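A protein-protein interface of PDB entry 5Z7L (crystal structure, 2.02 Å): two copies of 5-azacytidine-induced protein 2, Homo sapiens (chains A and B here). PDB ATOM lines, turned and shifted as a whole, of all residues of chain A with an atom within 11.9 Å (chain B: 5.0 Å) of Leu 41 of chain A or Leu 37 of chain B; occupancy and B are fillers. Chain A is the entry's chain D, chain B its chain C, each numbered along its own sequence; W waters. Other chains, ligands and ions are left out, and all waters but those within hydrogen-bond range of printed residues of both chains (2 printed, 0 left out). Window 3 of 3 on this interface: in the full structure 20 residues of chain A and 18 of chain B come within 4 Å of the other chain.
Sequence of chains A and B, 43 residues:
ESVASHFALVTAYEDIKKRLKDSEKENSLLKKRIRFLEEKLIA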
ATOM      1  N   LEU A  29      -5.219 -19.558 -15.290  1.00  0.00           N
ATOM      2  CA  LEU A  29      -4.553 -20.578 -14.482  1.00  0.00           C
ATOM      3  C   LEU A  29      -3.127 -20.833 -14.959  1.00  0.00           C
ATOM      4  O   LEU A  29      -2.223 -21.101 -14.149  1.00  0.00           O
ATOM      5  CB  LEU A  29      -5.360 -21.874 -14.521  1.00  0.00           C
ATOM      6  CG  LEU A  29      -6.771 -21.768 -13.928  1.00  0.00           C
ATOM      7  CD1 LEU A  29      -7.586 -23.034 -14.245  1.00  0.00           C
ATOM      8  CD2 LEU A  29      -6.694 -21.518 -12.417  1.00  0.00           C
ATOM      9  N   LEU A  30      -2.899 -20.778 -16.264  1.00  0.00           N
ATOM     10  CA  LEU A  30      -1.535 -20.940 -16.759  1.00  0.00           C
ATOM     11  C   LEU A  30      -0.647 -19.780 -16.310  1.00  0.00           C
ATOM     12  O   LEU A  30       0.520 -19.988 -15.972  1.00  0.00           O
ATOM     13  CB  LEU A  30      -1.539 -21.062 -18.279  1.00  0.00           C
ATOM     14  CG  LEU A  30      -2.351 -22.227 -18.831  1.00  0.00           C
ATOM     15  CD1 LEU A  30      -2.455 -22.098 -20.358  1.00  0.00           C
ATOM     16  CD2 LEU A  30      -1.734 -23.561 -18.403  1.00  0.00           C
ATOM     17  N   LYS A  31      -1.176 -18.553 -16.293  1.00  0.00           N
ATOM     18  CA  LYS A  31      -0.392 -17.429 -15.776  1.00  0.00           C
ATOM     19  C   LYS A  31      -0.044 -17.610 -14.301  1.00  0.00           C
ATOM     20  O   LYS A  31       1.054 -17.240 -13.868  1.00  0.00           O
ATOM     21  CB  LYS A  31      -1.141 -16.110 -15.981  1.00  0.00           C
ATOM     22  CG  LYS A  31      -1.248 -15.698 -17.439  1.00  0.00           C
ATOM     23  CD  LYS A  31      -2.209 -14.502 -17.596  1.00  0.00           C
ATOM     24  CE  LYS A  31      -2.135 -13.931 -18.987  1.00  0.00           C
ATOM     25  NZ  LYS A  31      -3.230 -12.941 -19.269  1.00  0.00           N
ATOM     26  N   LYS A  32      -0.974 -18.146 -13.503  1.00  0.00           N
ATOM     27  CA  LYS A  32      -0.691 -18.397 -12.092  1.00  0.00           C
ATOM     28  C   LYS A  32       0.437 -19.410 -11.940  1.00  0.00           C
ATOM     29  O   LYS A  32       1.345 -19.237 -11.120  1.00  0.00           O
ATOM     30  CB  LYS A  32      -1.956 -18.904 -11.392  1.00  0.00           C
ATOM     31  CG  LYS A  32      -2.267 -18.269 -10.059  1.00  0.00           C
ATOM     32  CD  LYS A  32      -1.996 -19.208  -8.904  1.00  0.00           C
ATOM     33  CE  LYS A  32      -3.264 -19.821  -8.304  1.00  0.00           C
ATOM     34  NZ  LYS A  32      -3.936 -20.749  -9.276  1.00  0.00           N
ATOM     35  N   ARG A  33       0.372 -20.480 -12.724  1.00  0.00           N
ATOM     36  CA  ARG A  33       1.387 -21.522 -12.693  1.00  0.00           C
ATOM     37  C   ARG A  33       2.755 -20.964 -13.065  1.00  0.00           C
ATOM     38  O   ARG A  33       3.767 -21.285 -12.428  1.00  0.00           O
ATOM     39  CB  ARG A  33       0.968 -22.646 -13.652  1.00  0.00           C
ATOM     40  CG  ARG A  33       2.027 -23.727 -13.914  1.00  0.00           C
ATOM     41  CD  ARG A  33       2.380 -24.535 -12.653  1.00  0.00           C
ATOM     42  NE  ARG A  33       3.341 -25.593 -12.968  1.00  0.00           N
ATOM     43  CZ  ARG A  33       4.256 -26.076 -12.127  1.00  0.00           C
ATOM     44  NH1 ARG A  33       4.350 -25.625 -10.880  1.00  0.00           N
ATOM     45  NH2 ARG A  33       5.085 -27.024 -12.537  1.00  0.00           N
ATOM     46  N   ILE A  34       2.803 -20.151 -14.122  1.00  0.00           N
ATOM     47  CA  ILE A  34       4.029 -19.458 -14.512  1.00  0.00           C
ATOM     48  C   ILE A  34       4.568 -18.620 -13.357  1.00  0.00           C
ATOM     49  O   ILE A  34       5.765 -18.661 -13.039  1.00  0.00           O
ATOM     50  CB  ILE A  34       3.772 -18.589 -15.755  1.00  0.00           C
ATOM     51  CG1 ILE A  34       3.699 -19.476 -16.997  1.00  0.00           C
ATOM     52  CG2 ILE A  34       4.875 -17.533 -15.901  1.00  0.00           C
ATOM     53  CD1 ILE A  34       2.920 -18.893 -18.159  1.00  0.00           C
ATOM     54  N   ARG A  35       3.701 -17.829 -12.722  1.00  0.00           N
ATOM     55  CA  ARG A  35       4.158 -16.973 -11.627  1.00  0.00           C
ATOM     56  C   ARG A  35       4.769 -17.801 -10.503  1.00  0.00           C
ATOM     57  O   ARG A  35       5.841 -17.463  -9.988  1.00  0.00           O
ATOM     58  CB  ARG A  35       3.002 -16.116 -11.102  1.00  0.00           C
ATOM     59  CG  ARG A  35       2.550 -15.024 -12.085  1.00  0.00           C
ATOM     60  CD  ARG A  35       1.762 -13.913 -11.378  1.00  0.00           C
ATOM     61  NE  ARG A  35       0.684 -14.438 -10.545  1.00  0.00           N
ATOM     62  CZ  ARG A  35      -0.537 -14.729 -10.987  1.00  0.00           C
ATOM     63  NH1 ARG A  35      -0.851 -14.540 -12.269  1.00  0.00           N
ATOM     64  NH2 ARG A  35      -1.448 -15.202 -10.143  1.00  0.00           N
ATOM     65  N   PHE A  36       4.097 -18.894 -10.113  1.00  0.00           N
ATOM     66  CA  PHE A  36       4.665 -19.825  -9.135  1.00  0.00           C
ATOM     67  C   PHE A  36       6.028 -20.338  -9.589  1.00  0.00           C
ATOM     68  O   PHE A  36       6.979 -20.401  -8.801  1.00  0.00           O
ATOM     69  CB  PHE A  36       3.725 -21.020  -8.910  1.00  0.00           C
ATOM     70  CG  PHE A  36       2.639 -20.770  -7.898  1.00  0.00           C
ATOM     71  CD1 PHE A  36       2.944 -20.307  -6.622  1.00  0.00           C
ATOM     72  CD2 PHE A  36       1.314 -21.005  -8.218  1.00  0.00           C
ATOM     73  CE1 PHE A  36       1.948 -20.077  -5.696  1.00  0.00           C
ATOM     74  CE2 PHE A  36       0.310 -20.779  -7.291  1.00  0.00           C
ATOM     75  CZ  PHE A  36       0.626 -20.317  -6.030  1.00  0.00           C
ATOM     76  N   LEU A  37       6.135 -20.765 -10.846  1.00  0.00           N
ATOM     77  CA  LEU A  37       7.425 -21.275 -11.302  1.00  0.00           C
ATOM     78  C   LEU A  37       8.484 -20.179 -11.284  1.00  0.00           C
ATOM     79  O   LEU A  37       9.640 -20.431 -10.928  1.00  0.00           O
ATOM     80  CB  LEU A  37       7.299 -21.886 -12.695  1.00  0.00           C
ATOM     81  CG  LEU A  37       6.656 -23.272 -12.803  1.00  0.00           C
ATOM     82  CD1 LEU A  37       6.057 -23.485 -14.202  1.00  0.00           C
ATOM     83  CD2 LEU A  37       7.665 -24.385 -12.471  1.00  0.00           C
ATOM     84  N   GLU A  38       8.114 -18.953 -11.661  1.00  0.00           N
ATOM     85  CA  GLU A  38       9.111 -17.890 -11.702  1.00  0.00           C
ATOM     86  C   GLU A  38       9.548 -17.479 -10.300  1.00  0.00           C
ATOM     87  O   GLU A  38      10.718 -17.145 -10.088  1.00  0.00           O
ATOM     88  CB  GLU A  38       8.569 -16.684 -12.470  1.00  0.00           C
ATOM     89  CG  GLU A  38       8.547 -16.923 -13.948  1.00  0.00           C
ATOM     90  CD  GLU A  38       7.676 -15.947 -14.703  1.00  0.00           C
ATOM     91  OE1 GLU A  38       6.808 -15.285 -14.090  1.00  0.00           O
ATOM     92  OE2 GLU A  38       7.870 -15.846 -15.923  1.00  0.00           O
ATOM     93  N   GLU A  39       8.634 -17.507  -9.331  1.00  0.00           N
ATOM     94  CA  GLU A  39       9.032 -17.244  -7.955  1.00  0.00           C
ATOM     95  C   GLU A  39      10.004 -18.310  -7.463  1.00  0.00           C
ATOM     96  O   GLU A  39      10.949 -18.007  -6.720  1.00  0.00           O
ATOM     97  CB  GLU A  39       7.794 -17.170  -7.067  1.00  0.00           C
ATOM     98  CG  GLU A  39       8.057 -16.631  -5.666  1.00  0.00           C
ATOM     99  CD  GLU A  39       6.837 -16.733  -4.764  1.00  0.00           C
ATOM    100  OE1 GLU A  39       5.787 -17.230  -5.229  1.00  0.00           O
ATOM    101  OE2 GLU A  39       6.932 -16.316  -3.588  1.00  0.00           O
ATOM    102  N   LYS A  40       9.806 -19.561  -7.890  1.00  0.00           N
ATOM    103  CA  LYS A  40      10.680 -20.652  -7.460  1.00  0.00           C
ATOM    104  C   LYS A  40      12.049 -20.570  -8.134  1.00  0.00           C
ATOM    105  O   LYS A  40      13.076 -20.834  -7.499  1.00  0.00           O
ATOM    106  CB  LYS A  40       9.987 -21.982  -7.750  1.00  0.00           C
ATOM    107  CG  LYS A  40      10.828 -23.245  -7.617  1.00  0.00           C
ATOM    108  CD  LYS A  40       9.890 -24.464  -7.493  1.00  0.00           C
ATOM    109  CE  LYS A  40      10.615 -25.793  -7.730  1.00  0.00           C
ATOM    110  NZ  LYS A  40       9.658 -26.891  -8.116  1.00  0.00           N
ATOM    111  N   LEU A  41      12.092 -20.156  -9.407  1.00  0.00           N
ATOM    112  CA  LEU A  41      13.321 -20.214 -10.191  1.00  0.00           C
ATOM    113  C   LEU A  41      14.080 -18.895 -10.268  1.00  0.00           C
ATOM    114  O   LEU A  41      15.287 -18.913 -10.533  1.00  0.00           O
ATOM    115  CB  LEU A  41      13.016 -20.687 -11.620  1.00  0.00           C
ATOM    116  CG  LEU A  41      12.623 -22.162 -11.694  1.00  0.00           C
ATOM    117  CD1 LEU A  41      11.779 -22.479 -12.937  1.00  0.00           C
ATOM    118  CD2 LEU A  41      13.883 -23.045 -11.628  1.00  0.00           C
ATOM    119  N   ILE A  42      13.422 -17.754 -10.082  1.00  0.00           N
ATOM    120  CA  ILE A  42      14.034 -16.451 -10.345  1.00  0.00           C
ATOM    121  C   ILE A  42      13.887 -15.594  -9.091  1.00  0.00           C
ATOM    122  O   ILE A  42      12.804 -15.075  -8.801  1.00  0.00           O
ATOM    123  CB  ILE A  42      13.431 -15.767 -11.579  1.00  0.00           C
ATOM    124  CG1 ILE A  42      13.326 -16.795 -12.718  1.00  0.00           C
ATOM    125  CG2 ILE A  42      14.285 -14.538 -11.993  1.00  0.00           C
ATOM    126  CD1 ILE A  42      12.589 -16.337 -13.953  1.00  0.00           C
ATOM    127  N   ALA A  43      14.972 -15.442  -8.343  1.00  0.00           N
ATOM    128  CA  ALA A  43      14.918 -14.698  -7.087  1.00  0.00           C
ATOM    129  C   ALA A  43      15.832 -13.470  -7.115  1.00  0.00           C
ATOM    130  O   ALA A  43      15.376 -12.344  -7.323  1.00  0.00           O
ATOM    131  CB  ALA A  43      15.286 -15.607  -5.921  1.00  0.00           C
ATOM    132  OXT ALA A  43      17.048 -13.568  -6.935  1.00  0.00           O
ATOM    133  N   ARG B  33       5.948 -21.211 -22.350  1.00  0.00           N
ATOM    134  CA  ARG B  33       6.691 -20.655 -21.223  1.00  0.00           C
ATOM    135  C   ARG B  33       6.767 -21.655 -20.068  1.00  0.00           C
ATOM    136  O   ARG B  33       7.834 -21.865 -19.491  1.00  0.00           O
ATOM    137  CB  ARG B  33       6.041 -19.337 -20.789  1.00  0.00           C
ATOM    138  CG  ARG B  33       6.642 -18.718 -19.561  1.00  0.00           C
ATOM    139  CD  ARG B  33       8.020 -18.147 -19.848  1.00  0.00           C
ATOM    140  NE  ARG B  33       8.536 -17.461 -18.671  1.00  0.00           N
ATOM    141  CZ  ARG B  33       9.811 -17.158 -18.485  1.00  0.00           C
ATOM    142  NH1 ARG B  33      10.705 -17.488 -19.409  1.00  0.00           N
ATOM    143  NH2 ARG B  33      10.185 -16.538 -17.375  1.00  0.00           N
ATOM    144  N   ILE B  34       5.648 -22.302 -19.737  1.00  0.00           N
ATOM    145  CA  ILE B  34       5.641 -23.291 -18.658  1.00  0.00           C
ATOM    146  C   ILE B  34       6.648 -24.399 -18.957  1.00  0.00           C
ATOM    147  O   ILE B  34       7.467 -24.769 -18.109  1.00  0.00           O
ATOM    148  CB  ILE B  34       4.215 -23.846 -18.464  1.00  0.00           C
ATOM    149  CG1 ILE B  34       3.318 -22.779 -17.832  1.00  0.00           C
ATOM    150  CG2 ILE B  34       4.210 -25.129 -17.611  1.00  0.00           C
ATOM    151  CD1 ILE B  34       1.882 -23.185 -17.734  1.00  0.00           C
ATOM    152  N   ARG B  35       6.618 -24.918 -20.184  1.00  0.00           N
ATOM    153  CA  ARG B  35       7.538 -25.981 -20.565  1.00  0.00           C
ATOM    154  C   ARG B  35       8.984 -25.516 -20.458  1.00  0.00           C
ATOM    155  O   ARG B  35       9.846 -26.260 -19.981  1.00  0.00           O
ATOM    156  CB  ARG B  35       7.226 -26.467 -21.983  1.00  0.00           C
ATOM    157  CG  ARG B  35       6.265 -27.666 -22.056  1.00  0.00           C
ATOM    158  CD  ARG B  35       6.241 -28.304 -23.459  1.00  0.00           C
ATOM    159  NE  ARG B  35       5.642 -27.406 -24.448  1.00  0.00           N
ATOM    160  CZ  ARG B  35       4.332 -27.189 -24.584  1.00  0.00           C
ATOM    161  NH1 ARG B  35       3.451 -27.824 -23.804  1.00  0.00           N
ATOM    162  NH2 ARG B  35       3.901 -26.337 -25.510  1.00  0.00           N
ATOM    163  N   PHE B  36       9.269 -24.283 -20.882  1.00  0.00           N
ATOM    164  CA  PHE B  36      10.620 -23.759 -20.724  1.00  0.00           C
ATOM    165  C   PHE B  36      11.024 -23.720 -19.254  1.00  0.00           C
ATOM    166  O   PHE B  36      12.149 -24.091 -18.895  1.00  0.00           O
ATOM    167  CB  PHE B  36      10.730 -22.362 -21.336  1.00  0.00           C
ATOM    168  CG  PHE B  36      11.996 -21.649 -20.954  1.00  0.00           C
ATOM    169  CD1 PHE B  36      12.046 -20.840 -19.834  1.00  0.00           C
ATOM    170  CD2 PHE B  36      13.147 -21.799 -21.716  1.00  0.00           C
ATOM    171  CE1 PHE B  36      13.217 -20.200 -19.477  1.00  0.00           C
ATOM    172  CE2 PHE B  36      14.317 -21.150 -21.365  1.00  0.00           C
ATOM    173  CZ  PHE B  36      14.351 -20.360 -20.244  1.00  0.00           C
ATOM    174  N   LEU B  37      10.130 -23.237 -18.387  1.00  0.00           N
ATOM    175  CA  LEU B  37      10.457 -23.150 -16.960  1.00  0.00           C
ATOM    176  C   LEU B  37      10.564 -24.528 -16.321  1.00  0.00           C
ATOM    177  O   LEU B  37      11.461 -24.769 -15.505  1.00  0.00           O
ATOM    178  CB  LEU B  37       9.409 -22.319 -16.232  1.00  0.00           C
ATOM    179  CG  LEU B  37       9.389 -20.857 -16.659  1.00  0.00           C
ATOM    180  CD1 LEU B  37       8.100 -20.182 -16.192  1.00  0.00           C
ATOM    181  CD2 LEU B  37      10.620 -20.147 -16.131  1.00  0.00           C
ATOM    182  N   GLU B  38       9.657 -25.450 -16.672  1.00  0.00           N
ATOM    183  CA  GLU B  38       9.731 -26.793 -16.099  1.00  0.00           C
ATOM    184  C   GLU B  38      11.014 -27.494 -16.516  1.00  0.00           C
ATOM    185  O   GLU B  38      11.581 -28.270 -15.740  1.00  0.00           O
ATOM    186  CB  GLU B  38       8.494 -27.615 -16.489  1.00  0.00           C
ATOM    187  CG  GLU B  38       7.237 -27.082 -15.789  1.00  0.00           C
ATOM    188  CD  GLU B  38       5.984 -27.879 -16.079  1.00  0.00           C
ATOM    189  OE1 GLU B  38       5.897 -28.508 -17.161  1.00  0.00           O
ATOM    190  OE2 GLU B  38       5.071 -27.858 -15.219  1.00  0.00           O
ATOM    191  N   GLU B  39      11.501 -27.221 -17.734  1.00  0.00           N
ATOM    192  CA  GLU B  39      12.815 -27.729 -18.129  1.00  0.00           C
ATOM    193  C   GLU B  39      13.896 -27.230 -17.180  1.00  0.00           C
ATOM    194  O   GLU B  39      14.843 -27.954 -16.863  1.00  0.00           O
ATOM    195  CB  GLU B  39      13.154 -27.318 -19.565  1.00  0.00           C
ATOM    196  CG  GLU B  39      12.387 -28.060 -20.657  1.00  0.00           C
ATOM    197  CD  GLU B  39      12.418 -27.312 -21.995  1.00  0.00           C
ATOM    198  OE1 GLU B  39      11.601 -27.636 -22.887  1.00  0.00           O
ATOM    199  OE2 GLU B  39      13.267 -26.402 -22.153  1.00  0.00           O
ATOM    200  N   LYS B  40      13.777 -25.993 -16.708  1.00  0.00           N
ATOM    201  CA  LYS B  40      14.777 -25.497 -15.771  1.00  0.00           C
ATOM    202  C   LYS B  40      14.702 -26.219 -14.430  1.00  0.00           C
ATOM    203  O   LYS B  40      15.674 -26.201 -13.673  1.00  0.00           O
ATOM    204  CB  LYS B  40      14.622 -23.984 -15.601  1.00  0.00           C
ATOM    205  CG  LYS B  40      14.910 -23.213 -16.913  1.00  0.00           C
ATOM    206  CD  LYS B  40      16.280 -23.585 -17.514  1.00  0.00           C
ATOM    207  CE  LYS B  40      16.336 -23.331 -19.029  1.00  0.00           C
ATOM    208  NZ  LYS B  40      15.112 -23.830 -19.753  1.00  0.00           N
ATOM    209  N   LEU B  41      13.584 -26.870 -14.128  1.00  0.00           N
ATOM    210  CA  LEU B  41      13.504 -27.779 -12.990  1.00  0.00           C
ATOM    211  C   LEU B  41      13.510 -29.232 -13.425  1.00  0.00           C
ATOM    212  O   LEU B  41      12.807 -30.038 -12.868  1.00  0.00           O
ATOM    213  CB  LEU B  41      12.288 -27.465 -12.114  1.00  0.00           C
ATOM    214  CG  LEU B  41      10.821 -27.213 -12.508  1.00  0.00           C
ATOM    215  CD1 LEU B  41      10.088 -28.444 -13.000  1.00  0.00           C
ATOM    216  CD2 LEU B  41      10.111 -26.699 -11.292  1.00  0.00           C
HETATM  217  O   HOH W   1       2.353 -27.171 -15.017  1.00  0.00           O
HETATM  218  O   HOH W   2       7.265 -14.761 -17.996  1.00  0.00           O
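The guanidinium group (NH2) of Arg 33 of chain B is in salt-bridge range of the side-chain carboxylate (OE2) of Glu 38 of chain A (2.8 Å).
The side-chain carboxylate (OE2) of Glu 38 of chain B is in salt-bridge range of the guanidinium group (NH2) of Arg 33 of chain A, 2.8 Å away.
Leu 30 of chain A touches Ile 34 of chain B.
Ile 34 of chain B touches Arg 33 of chain A (CD1 to CG, 3.9 Å).
Ile 34 of chain A touches Arg 33 of chain B.
Ile 34 of chain A touches Ile 34 of chain B.
CB of Leu 37 of chain A touches CD1 of Leu 37 of chain B, 3.97 Å away.
Leu 37 of chain A touches Leu 41 of chain B (CD2 to CD2, 3.6 Å).
Leu 37 of chain B touches Glu 38 of chain A.
NZ of Lys 40 of chain A touches CD2 of Leu 41 of chain B, 3.2 Å away.
O of Leu 37 of chain B touches CD1 of Leu 41 of chain A (3.5 Å).
Of the printed residues of chain B, Ile 34 of chain A touches Arg 33 and Ile 34.
Printed residues of chain B within 4 Å of Glu 38 of chain A: Arg 33 (2.8 Å) and Leu 37 (3.98 Å).
Of the printed residues of chain B, Lys 40 of chain A touches Leu 41 (3.2 Å).
Of the printed residues of chain B, Leu 41 of chain A touches Leu 37.
Arg 33 of chain B touches just these residues of chain A: Ile 34 (3.98 Å) and Glu 38 (2.8 Å).
Ile 34 of chain B touches just these residues of chain A: Leu 30, Arg 33 and Ile 34.
Arg 35 of chain B touches none of the printed residues of chain A.
No residue of chain A comes within 4 Å of Phe 36 of chain B.
Of the printed residues of chain A, Leu 37 of chain B touches Leu 37 (3.97 Å), Glu 38 (3.98 Å) and Leu 41 (3.5 Å).
Printed residues of chain A within 4 Å of Glu 38 of chain B: Arg 33.
Glu 39 of chain B touches none of the printed residues of chain A.
Leu 41 of chain B touches just these residues of chain A: Leu 37 (3.6 Å) and Lys 40 (3.2 Å).
The nearest printed residue of chain A that does not touch Leu 37 of chain B is Ile 34 of chain A (4.2 Å).
Hydrophobic or aromatic side chains of chain B within 4 Å of the printed part of chain A: Ile 34, Leu 37 and Leu 41.
Along chain B the printed residues that touch a printed residue of chain A span positions 33 to 41.
Hydrophobic or aromatic side chains of chain A that line the printed part of chain B: Leu 30, Ile 34, Leu 37 and Leu 41.
Among the printed residues, 11 pairs touch across the chains.
Arg 33 of chain A touches Ile 34 of chain B, and with the chains exchanged Ile 34 of chain A touches Arg 33 of chain B.
Ile 34 of chain A touches its own counterpart, Ile 34 of chain B.
Leu 37 of chain A touches its own counterpart, Leu 37 of chain B.
Glu 38 of chain A touches Leu 37 of chain B, but with the chains exchanged Leu 37 of chain A does not touch Glu 38 of chain B (4.1 Å).
Water W2 bridges OE2 of Glu 38 of chain A (2.4 Å) and NE of Arg 33 of chain B (3.1 Å).
Water W1 bridges NE of Arg 33 of chain A (2.8 Å) and OE2 of Glu 38 of chain B (2.8 Å).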
